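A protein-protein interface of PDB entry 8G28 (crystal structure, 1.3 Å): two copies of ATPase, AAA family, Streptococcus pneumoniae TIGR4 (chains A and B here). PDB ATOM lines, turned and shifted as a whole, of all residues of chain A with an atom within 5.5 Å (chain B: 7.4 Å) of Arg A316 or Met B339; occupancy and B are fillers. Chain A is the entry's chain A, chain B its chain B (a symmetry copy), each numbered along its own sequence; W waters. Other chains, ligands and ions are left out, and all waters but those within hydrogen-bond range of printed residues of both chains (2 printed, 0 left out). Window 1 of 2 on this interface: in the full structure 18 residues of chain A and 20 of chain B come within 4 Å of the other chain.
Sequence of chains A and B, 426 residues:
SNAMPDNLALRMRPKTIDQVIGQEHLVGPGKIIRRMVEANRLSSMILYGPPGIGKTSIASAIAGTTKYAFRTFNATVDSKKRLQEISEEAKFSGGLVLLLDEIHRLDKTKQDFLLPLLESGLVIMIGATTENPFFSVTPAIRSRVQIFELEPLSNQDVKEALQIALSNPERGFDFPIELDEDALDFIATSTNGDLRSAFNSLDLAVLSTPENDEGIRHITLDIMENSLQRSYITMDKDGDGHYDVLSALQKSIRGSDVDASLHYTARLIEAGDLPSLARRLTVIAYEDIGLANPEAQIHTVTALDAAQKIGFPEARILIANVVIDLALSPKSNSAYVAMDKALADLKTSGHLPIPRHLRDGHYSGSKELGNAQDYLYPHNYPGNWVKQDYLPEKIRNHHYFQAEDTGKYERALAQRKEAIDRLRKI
The guanidinium group (NE) of Arg A316 is in salt-bridge range of the side-chain carboxylate (OD1) of Asp B340.
Of the 15 printed residues of chain B, 9 touch a printed residue of chain A.
Hydrophobic or aromatic side chains of chain B within 4 Å of the printed part of chain A: Val B283, Ala B335, Tyr B336, Ala B338, Met B339, Ala B342 and Leu B343.
Of the 15 printed residues of chain A, 8 touch a printed residue of chain B.
Hydrophobic or aromatic side chains of chain A that line the printed part of chain B: Leu A262, Ala A266, Ile A269, Ile A317 and Ala A320.
Among the printed residues, 17 pairs touch across the chains.
Among the printed residues, Asp or Glu carboxylates within 4 Å of a Lys or Arg side-chain nitrogen of the other chain: Arg A316 with Asp B340.
O of Ile A317 lies within hydrogen-bond range of ND2 of Asn A321 (2.9 Å).
O of Pro A313 lies within hydrogen-bond range of NH1 of Arg A316.
OH of Tyr B336 sits close to OD2 of Asp B340 (3.3 Å).
No position is printed for both chains.
Of the 17 pairs that touch across the chains among the printed residues, none has its exchanged pair printed and touching as well.
Met B339 touches Leu A262.
O of Leu A262 touches CB of Ala B342, 3.7 Å away.
O of Ala A266 touches CD2 of Leu B343, 3.6 Å away.
Arg A316 touches Tyr B336 (NH2 to CE2, 3.5 Å).
Arg A316 touches Met B339 (O to CG, 3.5 Å).
Leu B343 touches Arg A316 (CD1 to CD, 3.8 Å).
Glu B287 touches Ile A317.
Ala A320 touches Ala B335 (CB to O, 3.5 Å).
Ala A320 touches Met B339 (CB to CB, 3.5 Å).
CB of Ala B335 touches ND2 of Asn A321, at 3.7 Å.
Printed residues of chain A within 4 Å of Met B339: Leu A262 (3.5 Å), Ala A266 (3.7 Å), Ile A269 (3.8 Å), Arg A316 (3.5 Å) and Ala A320 (3.5 Å).
No residue of chain B comes within 4 Å of Ala A315.
Of the printed residues of chain A, Val B283 touches Glu A314 (3.8 Å).
Of the printed residues of chain B, Asn A321 touches Ala B335 (3.7 Å).
Printed residues of chain B within 4 Å of Ile A269: Met B339.
Printed residues of chain B within 4 Å of Glu A314: Val B283 (3.8 Å).
Of the printed residues of chain A, Glu B287 touches Ile A317.
The nearest printed residue of chain B that does not touch Arg A316 is Ala B335 (6.1 Å).
The nearest printed residue of chain A that does not touch Ala B338 is Ala A320 (5.9 Å).
Water W2 bridges the guanidinium group of Arg A316 (3.0 Å) and the side-chain hydroxyl of Tyr B336 (3.5 Å).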
ATOM      1  N   LEU A 262      -2.491  12.547  27.913  1.00  0.00           N
ATOM      2  CA  LEU A 262      -2.433  11.462  26.899  1.00  0.00           C
ATOM      3  C   LEU A 262      -2.511  10.094  27.583  1.00  0.00           C
ATOM      4  O   LEU A 262      -3.082   9.172  26.989  1.00  0.00           O
ATOM      5  CB  LEU A 262      -1.147  11.624  26.089  1.00  0.00           C
ATOM      6  CG  LEU A 262      -1.174  12.763  25.074  1.00  0.00           C
ATOM      7  CD1 LEU A 262       0.225  13.064  24.572  1.00  0.00           C
ATOM      8  CD2 LEU A 262      -2.111  12.441  23.920  1.00  0.00           C
ATOM      9  N   THR A 265      -6.167   9.497  28.472  1.00  0.00           N
ATOM     10  CA  THR A 265      -6.869   9.278  27.188  1.00  0.00           C
ATOM     11  C   THR A 265      -6.561   7.865  26.682  1.00  0.00           C
ATOM     12  O   THR A 265      -7.491   7.183  26.235  1.00  0.00           O
ATOM     13  CB  THR A 265      -6.451  10.335  26.161  1.00  0.00           C
ATOM     14  OG1 THR A 265      -6.772  11.631  26.670  1.00  0.00           O
ATOM     15  CG2 THR A 265      -7.132  10.131  24.826  1.00  0.00           C
ATOM     16  N   ALA A 266      -5.298   7.446  26.753  1.00  0.00           N
ATOM     17  CA  ALA A 266      -4.923   6.090  26.281  1.00  0.00           C
ATOM     18  C   ALA A 266      -5.732   5.026  27.038  1.00  0.00           C
ATOM     19  O   ALA A 266      -6.215   4.067  26.407  1.00  0.00           O
ATOM     20  CB  ALA A 266      -3.437   5.878  26.450  1.00  0.00           C
ATOM     21  N   ILE A 269      -9.207   4.997  25.604  1.00  0.00           N
ATOM     22  CA  ILE A 269      -9.219   4.384  24.243  1.00  0.00           C
ATOM     23  C   ILE A 269      -9.132   2.856  24.365  1.00  0.00           C
ATOM     24  O   ILE A 269      -9.891   2.165  23.663  1.00  0.00           O
ATOM     25  CB  ILE A 269      -8.100   4.991  23.378  1.00  0.00           C
ATOM     26  CG1 ILE A 269      -8.441   6.448  23.059  1.00  0.00           C
ATOM     27  CG2 ILE A 269      -7.847   4.161  22.125  1.00  0.00           C
ATOM     28  CD1 ILE A 269      -7.344   7.207  22.364  1.00  0.00           C
ATOM     29  N   GLY A 311     -14.582   5.685  13.995  1.00  0.00           N
ATOM     30  CA  GLY A 311     -14.456   4.606  14.995  1.00  0.00           C
ATOM     31  C   GLY A 311     -13.008   4.223  15.253  1.00  0.00           C
ATOM     32  O   GLY A 311     -12.133   4.576  14.429  1.00  0.00           O
ATOM     33  N   PHE A 312     -12.748   3.569  16.388  1.00  0.00           N
ATOM     34  CA  PHE A 312     -11.389   3.028  16.650  1.00  0.00           C
ATOM     35  C   PHE A 312     -11.103   1.955  15.604  1.00  0.00           C
ATOM     36  O   PHE A 312     -12.026   1.294  15.128  1.00  0.00           O
ATOM     37  CB  PHE A 312     -11.281   2.487  18.079  1.00  0.00           C
ATOM     38  CG  PHE A 312     -11.397   3.540  19.153  1.00  0.00           C
ATOM     39  CD1 PHE A 312     -10.548   4.635  19.158  1.00  0.00           C
ATOM     40  CD2 PHE A 312     -12.329   3.424  20.173  1.00  0.00           C
ATOM     41  CE1 PHE A 312     -10.649   5.606  20.142  1.00  0.00           C
ATOM     42  CE2 PHE A 312     -12.420   4.391  21.162  1.00  0.00           C
ATOM     43  CZ  PHE A 312     -11.584   5.482  21.141  1.00  0.00           C
ATOM     44  N   PRO A 313      -9.822   1.687  15.259  1.00  0.00           N
ATOM     45  CA  PRO A 313      -8.674   2.355  15.879  1.00  0.00           C
ATOM     46  C   PRO A 313      -8.281   3.752  15.365  1.00  0.00           C
ATOM     47  O   PRO A 313      -7.645   4.482  16.110  1.00  0.00           O
ATOM     48  CB  PRO A 313      -7.521   1.391  15.556  1.00  0.00           C
ATOM     49  CG  PRO A 313      -7.923   0.765  14.239  1.00  0.00           C
ATOM     50  CD  PRO A 313      -9.424   0.599  14.348  1.00  0.00           C
ATOM     51  N   GLU A 314      -8.665   4.107  14.135  1.00  0.00           N
ATOM     52  CA  GLU A 314      -8.216   5.404  13.550  1.00  0.00           C
ATOM     53  C   GLU A 314      -8.695   6.599  14.385  1.00  0.00           C
ATOM     54  O   GLU A 314      -7.985   7.621  14.389  1.00  0.00           O
ATOM     55  CB  GLU A 314      -8.670   5.543  12.096  1.00  0.00           C
ATOM     56  CG  GLU A 314      -8.042   4.528  11.162  1.00  0.00           C
ATOM     57  CD  GLU A 314      -8.719   3.170  11.122  1.00  0.00           C
ATOM     58  OE1 GLU A 314      -9.709   2.961  11.869  1.00  0.00           O
ATOM     59  OE2 GLU A 314      -8.296   2.345  10.293  1.00  0.00           O
ATOM     60  N   ALA A 315      -9.824   6.487  15.082  1.00  0.00           N
ATOM     61  CA  ALA A 315     -10.319   7.613  15.905  1.00  0.00           C
ATOM     62  C   ALA A 315      -9.265   8.051  16.932  1.00  0.00           C
ATOM     63  O   ALA A 315      -9.293   9.206  17.343  1.00  0.00           O
ATOM     64  CB  ALA A 315     -11.596   7.210  16.593  1.00  0.00           C
ATOM     65  N   ARG A 316      -8.359   7.165  17.346  1.00  0.00           N
ATOM     66  CA  ARG A 316      -7.341   7.562  18.360  1.00  0.00           C
ATOM     67  C   ARG A 316      -6.487   8.723  17.830  1.00  0.00           C
ATOM     68  O   ARG A 316      -5.987   9.524  18.647  1.00  0.00           O
ATOM     69  CB  ARG A 316      -6.448   6.374  18.736  1.00  0.00           C
ATOM     70  CG  ARG A 316      -5.387   6.037  17.700  1.00  0.00           C
ATOM     71  CD  ARG A 316      -4.761   4.679  17.946  1.00  0.00           C
ATOM     72  NE  ARG A 316      -3.575   4.496  17.127  1.00  0.00           N
ATOM     73  CZ  ARG A 316      -3.580   4.206  15.830  1.00  0.00           C
ATOM     74  NH1 ARG A 316      -4.720   4.055  15.177  1.00  0.00           N
ATOM     75  NH2 ARG A 316      -2.433   4.077  15.186  1.00  0.00           N
ATOM     76  N   ILE A 317      -6.280   8.791  16.515  1.00  0.00           N
ATOM     77  CA  ILE A 317      -5.396   9.828  15.914  1.00  0.00           C
ATOM     78  C   ILE A 317      -6.096  11.190  16.003  1.00  0.00           C
ATOM     79  O   ILE A 317      -5.447  12.205  16.313  1.00  0.00           O
ATOM     80  CB  ILE A 317      -5.051   9.442  14.464  1.00  0.00           C
ATOM     81  CG1 ILE A 317      -4.466   8.029  14.388  1.00  0.00           C
ATOM     82  CG2 ILE A 317      -4.126  10.473  13.833  1.00  0.00           C
ATOM     83  CD1 ILE A 317      -4.328   7.476  12.988  1.00  0.00           C
ATOM     84  N   LEU A 318      -7.395  11.204  15.729  1.00  0.00           N
ATOM     85  CA  LEU A 318      -8.199  12.448  15.849  1.00  0.00           C
ATOM     86  C   LEU A 318      -8.207  12.905  17.315  1.00  0.00           C
ATOM     87  O   LEU A 318      -7.987  14.082  17.610  1.00  0.00           O
ATOM     88  CB  LEU A 318      -9.615  12.181  15.327  1.00  0.00           C
ATOM     89  CG  LEU A 318      -9.778  12.220  13.807  1.00  0.00           C
ATOM     90  CD1 LEU A 318      -8.946  11.170  13.095  1.00  0.00           C
ATOM     91  CD2 LEU A 318     -11.237  12.062  13.435  1.00  0.00           C
ATOM     92  N   ILE A 319      -8.462  11.969  18.220  1.00  0.00           N
ATOM     93  CA  ILE A 319      -8.503  12.290  19.673  1.00  0.00           C
ATOM     94  C   ILE A 319      -7.137  12.825  20.136  1.00  0.00           C
ATOM     95  O   ILE A 319      -7.116  13.740  20.965  1.00  0.00           O
ATOM     96  CB  ILE A 319      -8.958  11.048  20.453  1.00  0.00           C
ATOM     97  CG1 ILE A 319     -10.418  10.725  20.124  1.00  0.00           C
ATOM     98  CG2 ILE A 319      -8.749  11.231  21.942  1.00  0.00           C
ATOM     99  CD1 ILE A 319     -10.855   9.334  20.502  1.00  0.00           C
ATOM    100  N   ALA A 320      -6.033  12.262  19.647  1.00  0.00           N
ATOM    101  CA  ALA A 320      -4.690  12.747  20.052  1.00  0.00           C
ATOM    102  C   ALA A 320      -4.542  14.245  19.771  1.00  0.00           C
ATOM    103  O   ALA A 320      -3.979  14.983  20.609  1.00  0.00           O
ATOM    104  CB  ALA A 320      -3.642  11.970  19.302  1.00  0.00           C
ATOM    105  N   ASN A 321      -4.958  14.665  18.577  1.00  0.00           N
ATOM    106  CA  ASN A 321      -4.887  16.102  18.217  1.00  0.00           C
ATOM    107  C   ASN A 321      -5.695  16.941  19.218  1.00  0.00           C
ATOM    108  O   ASN A 321      -5.219  18.000  19.651  1.00  0.00           O
ATOM    109  CB  ASN A 321      -5.372  16.346  16.785  1.00  0.00           C
ATOM    110  CG  ASN A 321      -4.342  15.985  15.734  1.00  0.00           C
ATOM    111  OD1 ASN A 321      -3.587  16.847  15.289  1.00  0.00           O
ATOM    112  ND2 ASN A 321      -4.293  14.721  15.336  1.00  0.00           N
ATOM    113  N   VAL B 283      -8.308  10.634   7.908  1.00  0.00           N
ATOM    114  CA  VAL B 283      -7.197  10.114   8.740  1.00  0.00           C
ATOM    115  C   VAL B 283      -5.895  10.833   8.357  1.00  0.00           C
ATOM    116  O   VAL B 283      -5.176  11.284   9.269  1.00  0.00           O
ATOM    117  CB  VAL B 283      -7.097   8.586   8.611  1.00  0.00           C
ATOM    118  CG1 VAL B 283      -5.861   8.066   9.321  1.00  0.00           C
ATOM    119  CG2 VAL B 283      -8.348   7.910   9.144  1.00  0.00           C
ATOM    120  N   GLU B 287      -3.299  12.572  10.839  1.00  0.00           N
ATOM    121  CA  GLU B 287      -2.082  11.755  11.056  1.00  0.00           C
ATOM    122  C   GLU B 287      -0.839  12.453  10.494  1.00  0.00           C
ATOM    123  O   GLU B 287       0.200  12.462  11.169  1.00  0.00           O
ATOM    124  CB  GLU B 287      -2.257  10.408  10.356  1.00  0.00           C
ATOM    125  CG  GLU B 287      -1.015   9.534  10.381  1.00  0.00           C
ATOM    126  CD  GLU B 287      -1.176   8.163   9.743  1.00  0.00           C
ATOM    127  OE1 GLU B 287      -2.315   7.802   9.404  1.00  0.00           O
ATOM    128  OE2 GLU B 287      -0.150   7.480   9.554  1.00  0.00           O
ATOM    129  N   ASN B 333       3.720  14.513  12.199  1.00  0.00           N
ATOM    130  CA  ASN B 333       3.200  13.225  12.730  1.00  0.00           C
ATOM    131  C   ASN B 333       3.258  13.245  14.268  1.00  0.00           C
ATOM    132  O   ASN B 333       3.049  12.186  14.871  1.00  0.00           O
ATOM    133  CB  ASN B 333       3.962  12.027  12.156  1.00  0.00           C
ATOM    134  CG  ASN B 333       5.352  11.866  12.731  1.00  0.00           C
ATOM    135  OD1 ASN B 333       5.829  12.727  13.462  1.00  0.00           O
ATOM    136  ND2 ASN B 333       6.002  10.761  12.406  1.00  0.00           N
ATOM    137  N   SER B 334       3.444  14.418  14.885  1.00  0.00           N
ATOM    138  CA  SER B 334       3.721  14.460  16.346  1.00  0.00           C
ATOM    139  C   SER B 334       2.530  13.981  17.187  1.00  0.00           C
ATOM    140  O   SER B 334       2.763  13.282  18.184  1.00  0.00           O
ATOM    141  CB  SER B 334       4.226  15.817  16.780  1.00  0.00           C
ATOM    142  OG  SER B 334       3.254  16.831  16.637  1.00  0.00           O
ATOM    143  N   ALA B 335       1.301  14.339  16.827  1.00  0.00           N
ATOM    144  CA  ALA B 335       0.138  13.887  17.633  1.00  0.00           C
ATOM    145  C   ALA B 335      -0.014  12.366  17.522  1.00  0.00           C
ATOM    146  O   ALA B 335      -0.258  11.701  18.535  1.00  0.00           O
ATOM    147  CB  ALA B 335      -1.120  14.600  17.193  1.00  0.00           C
ATOM    148  N   TYR B 336       0.118  11.835  16.304  1.00  0.00           N
ATOM    149  CA  TYR B 336       0.021  10.371  16.078  1.00  0.00           C
ATOM    150  C   TYR B 336       1.049   9.641  16.949  1.00  0.00           C
ATOM    151  O   TYR B 336       0.679   8.706  17.687  1.00  0.00           O
ATOM    152  CB  TYR B 336       0.255  10.056  14.599  1.00  0.00           C
ATOM    153  CG  TYR B 336       0.358   8.587  14.278  1.00  0.00           C
ATOM    154  CD1 TYR B 336       1.542   7.889  14.454  1.00  0.00           C
ATOM    155  CD2 TYR B 336      -0.734   7.890  13.795  1.00  0.00           C
ATOM    156  CE1 TYR B 336       1.633   6.537  14.168  1.00  0.00           C
ATOM    157  CE2 TYR B 336      -0.657   6.543  13.489  1.00  0.00           C
ATOM    158  CZ  TYR B 336       0.528   5.860  13.682  1.00  0.00           C
ATOM    159  OH  TYR B 336       0.583   4.531  13.386  1.00  0.00           O
ATOM    160  N   VAL B 337       2.308  10.075  16.868  1.00  0.00           N
ATOM    161  CA  VAL B 337       3.409   9.432  17.641  1.00  0.00           C
ATOM    162  C   VAL B 337       3.106   9.510  19.141  1.00  0.00           C
ATOM    163  O   VAL B 337       3.272   8.503  19.852  1.00  0.00           O
ATOM    164  CB  VAL B 337       4.753  10.108  17.311  1.00  0.00           C
ATOM    165  CG1 VAL B 337       5.858   9.694  18.273  1.00  0.00           C
ATOM    166  CG2 VAL B 337       5.156   9.834  15.872  1.00  0.00           C
ATOM    167  N   ALA B 338       2.695  10.680  19.622  1.00  0.00           N
ATOM    168  CA  ALA B 338       2.482  10.847  21.077  1.00  0.00           C
ATOM    169  C   ALA B 338       1.405   9.889  21.585  1.00  0.00           C
ATOM    170  O   ALA B 338       1.526   9.345  22.678  1.00  0.00           O
ATOM    171  CB  ALA B 338       2.153  12.285  21.379  1.00  0.00           C
ATOM    172  N   MET B 339       0.361   9.688  20.774  1.00  0.00           N
ATOM    173  CA  MET B 339      -0.758   8.836  21.140  1.00  0.00           C
ATOM    174  C   MET B 339      -0.341   7.363  21.198  1.00  0.00           C
ATOM    175  O   MET B 339      -0.708   6.648  22.131  1.00  0.00           O
ATOM    176  CB  MET B 339      -1.897   9.045  20.137  1.00  0.00           C
ATOM    177  CG  MET B 339      -3.201   8.358  20.500  1.00  0.00           C
ATOM    178  SD  MET B 339      -4.140   9.224  21.992  1.00  0.00           S
ATOM    179  CE  MET B 339      -3.470   8.403  23.633  1.00  0.00           C
ATOM    180  N   ASP B 340       0.415   6.906  20.194  1.00  0.00           N
ATOM    181  CA  ASP B 340       0.839   5.511  20.144  1.00  0.00           C
ATOM    182  C   ASP B 340       1.906   5.239  21.213  1.00  0.00           C
ATOM    183  O   ASP B 340       1.938   4.109  21.732  1.00  0.00           O
ATOM    184  CB  ASP B 340       1.224   5.084  18.729  1.00  0.00           C
ATOM    185  CG  ASP B 340       0.000   4.775  17.879  1.00  0.00           C
ATOM    186  OD1 ASP B 340      -1.114   4.744  18.452  1.00  0.00           O
ATOM    187  OD2 ASP B 340       0.161   4.579  16.657  1.00  0.00           O
ATOM    188  N   LYS B 341       2.715   6.243  21.558  1.00  0.00           N
ATOM    189  CA  LYS B 341       3.671   6.114  22.688  1.00  0.00           C
ATOM    190  C   LYS B 341       2.873   5.916  23.984  1.00  0.00           C
ATOM    191  O   LYS B 341       3.214   5.028  24.787  1.00  0.00           O
ATOM    192  CB  LYS B 341       4.557   7.360  22.787  1.00  0.00           C
ATOM    193  CG  LYS B 341       5.544   7.349  23.947  1.00  0.00           C
ATOM    194  CD  LYS B 341       6.166   8.688  24.285  1.00  0.00           C
ATOM    195  CE  LYS B 341       7.169   9.184  23.268  1.00  0.00           C
ATOM    196  NZ  LYS B 341       7.954  10.330  23.790  1.00  0.00           N
ATOM    197  N   ALA B 342       1.830   6.721  24.183  1.00  0.00           N
ATOM    198  CA  ALA B 342       1.037   6.625  25.432  1.00  0.00           C
ATOM    199  C   ALA B 342       0.325   5.267  25.509  1.00  0.00           C
ATOM    200  O   ALA B 342       0.266   4.675  26.610  1.00  0.00           O
ATOM    201  CB  ALA B 342       0.064   7.771  25.518  1.00  0.00           C
ATOM    202  N   LEU B 343      -0.206   4.782  24.385  1.00  0.00           N
ATOM    203  CA  LEU B 343      -0.899   3.464  24.377  1.00  0.00           C
ATOM    204  C   LEU B 343       0.103   2.343  24.673  1.00  0.00           C
ATOM    205  O   LEU B 343      -0.251   1.417  25.437  1.00  0.00           O
ATOM    206  CB  LEU B 343      -1.596   3.259  23.030  1.00  0.00           C
ATOM    207  CG  LEU B 343      -2.893   4.050  22.867  1.00  0.00           C
ATOM    208  CD1 LEU B 343      -3.278   4.197  21.409  1.00  0.00           C
ATOM    209  CD2 LEU B 343      -4.022   3.404  23.659  1.00  0.00           C
ATOM    210  N   ALA B 344       1.313   2.437  24.117  1.00  0.00           N
ATOM    211  CA  ALA B 344       2.335   1.393  24.361  1.00  0.00           C
ATOM    212  C   ALA B 344       2.749   1.402  25.837  1.00  0.00           C
ATOM    213  O   ALA B 344       3.032   0.322  26.373  1.00  0.00           O
ATOM    214  CB  ALA B 344       3.523   1.604  23.458  1.00  0.00           C
ATOM    215  N   ASP B 345       2.771   2.579  26.463  1.00  0.00           N
ATOM    216  CA  ASP B 345       3.177   2.743  27.886  1.00  0.00           C
ATOM    217  C   ASP B 345       2.206   2.002  28.812  1.00  0.00           C
ATOM    218  O   ASP B 345       2.634   1.669  29.929  1.00  0.00           O
ATOM    219  CB  ASP B 345       3.236   4.218  28.291  1.00  0.00           C
ATOM    220  CG  ASP B 345       4.461   4.960  27.787  1.00  0.00           C
ATOM    221  OD1 ASP B 345       5.427   4.286  27.369  1.00  0.00           O
ATOM    222  OD2 ASP B 345       4.437   6.209  27.818  1.00  0.00           O
HETATM  223  O   HOH W   1      -2.017   7.631  17.151  1.00  0.00           O
HETATM  224  O   HOH W   2      -2.591   3.743  12.239  1.00  0.00           O
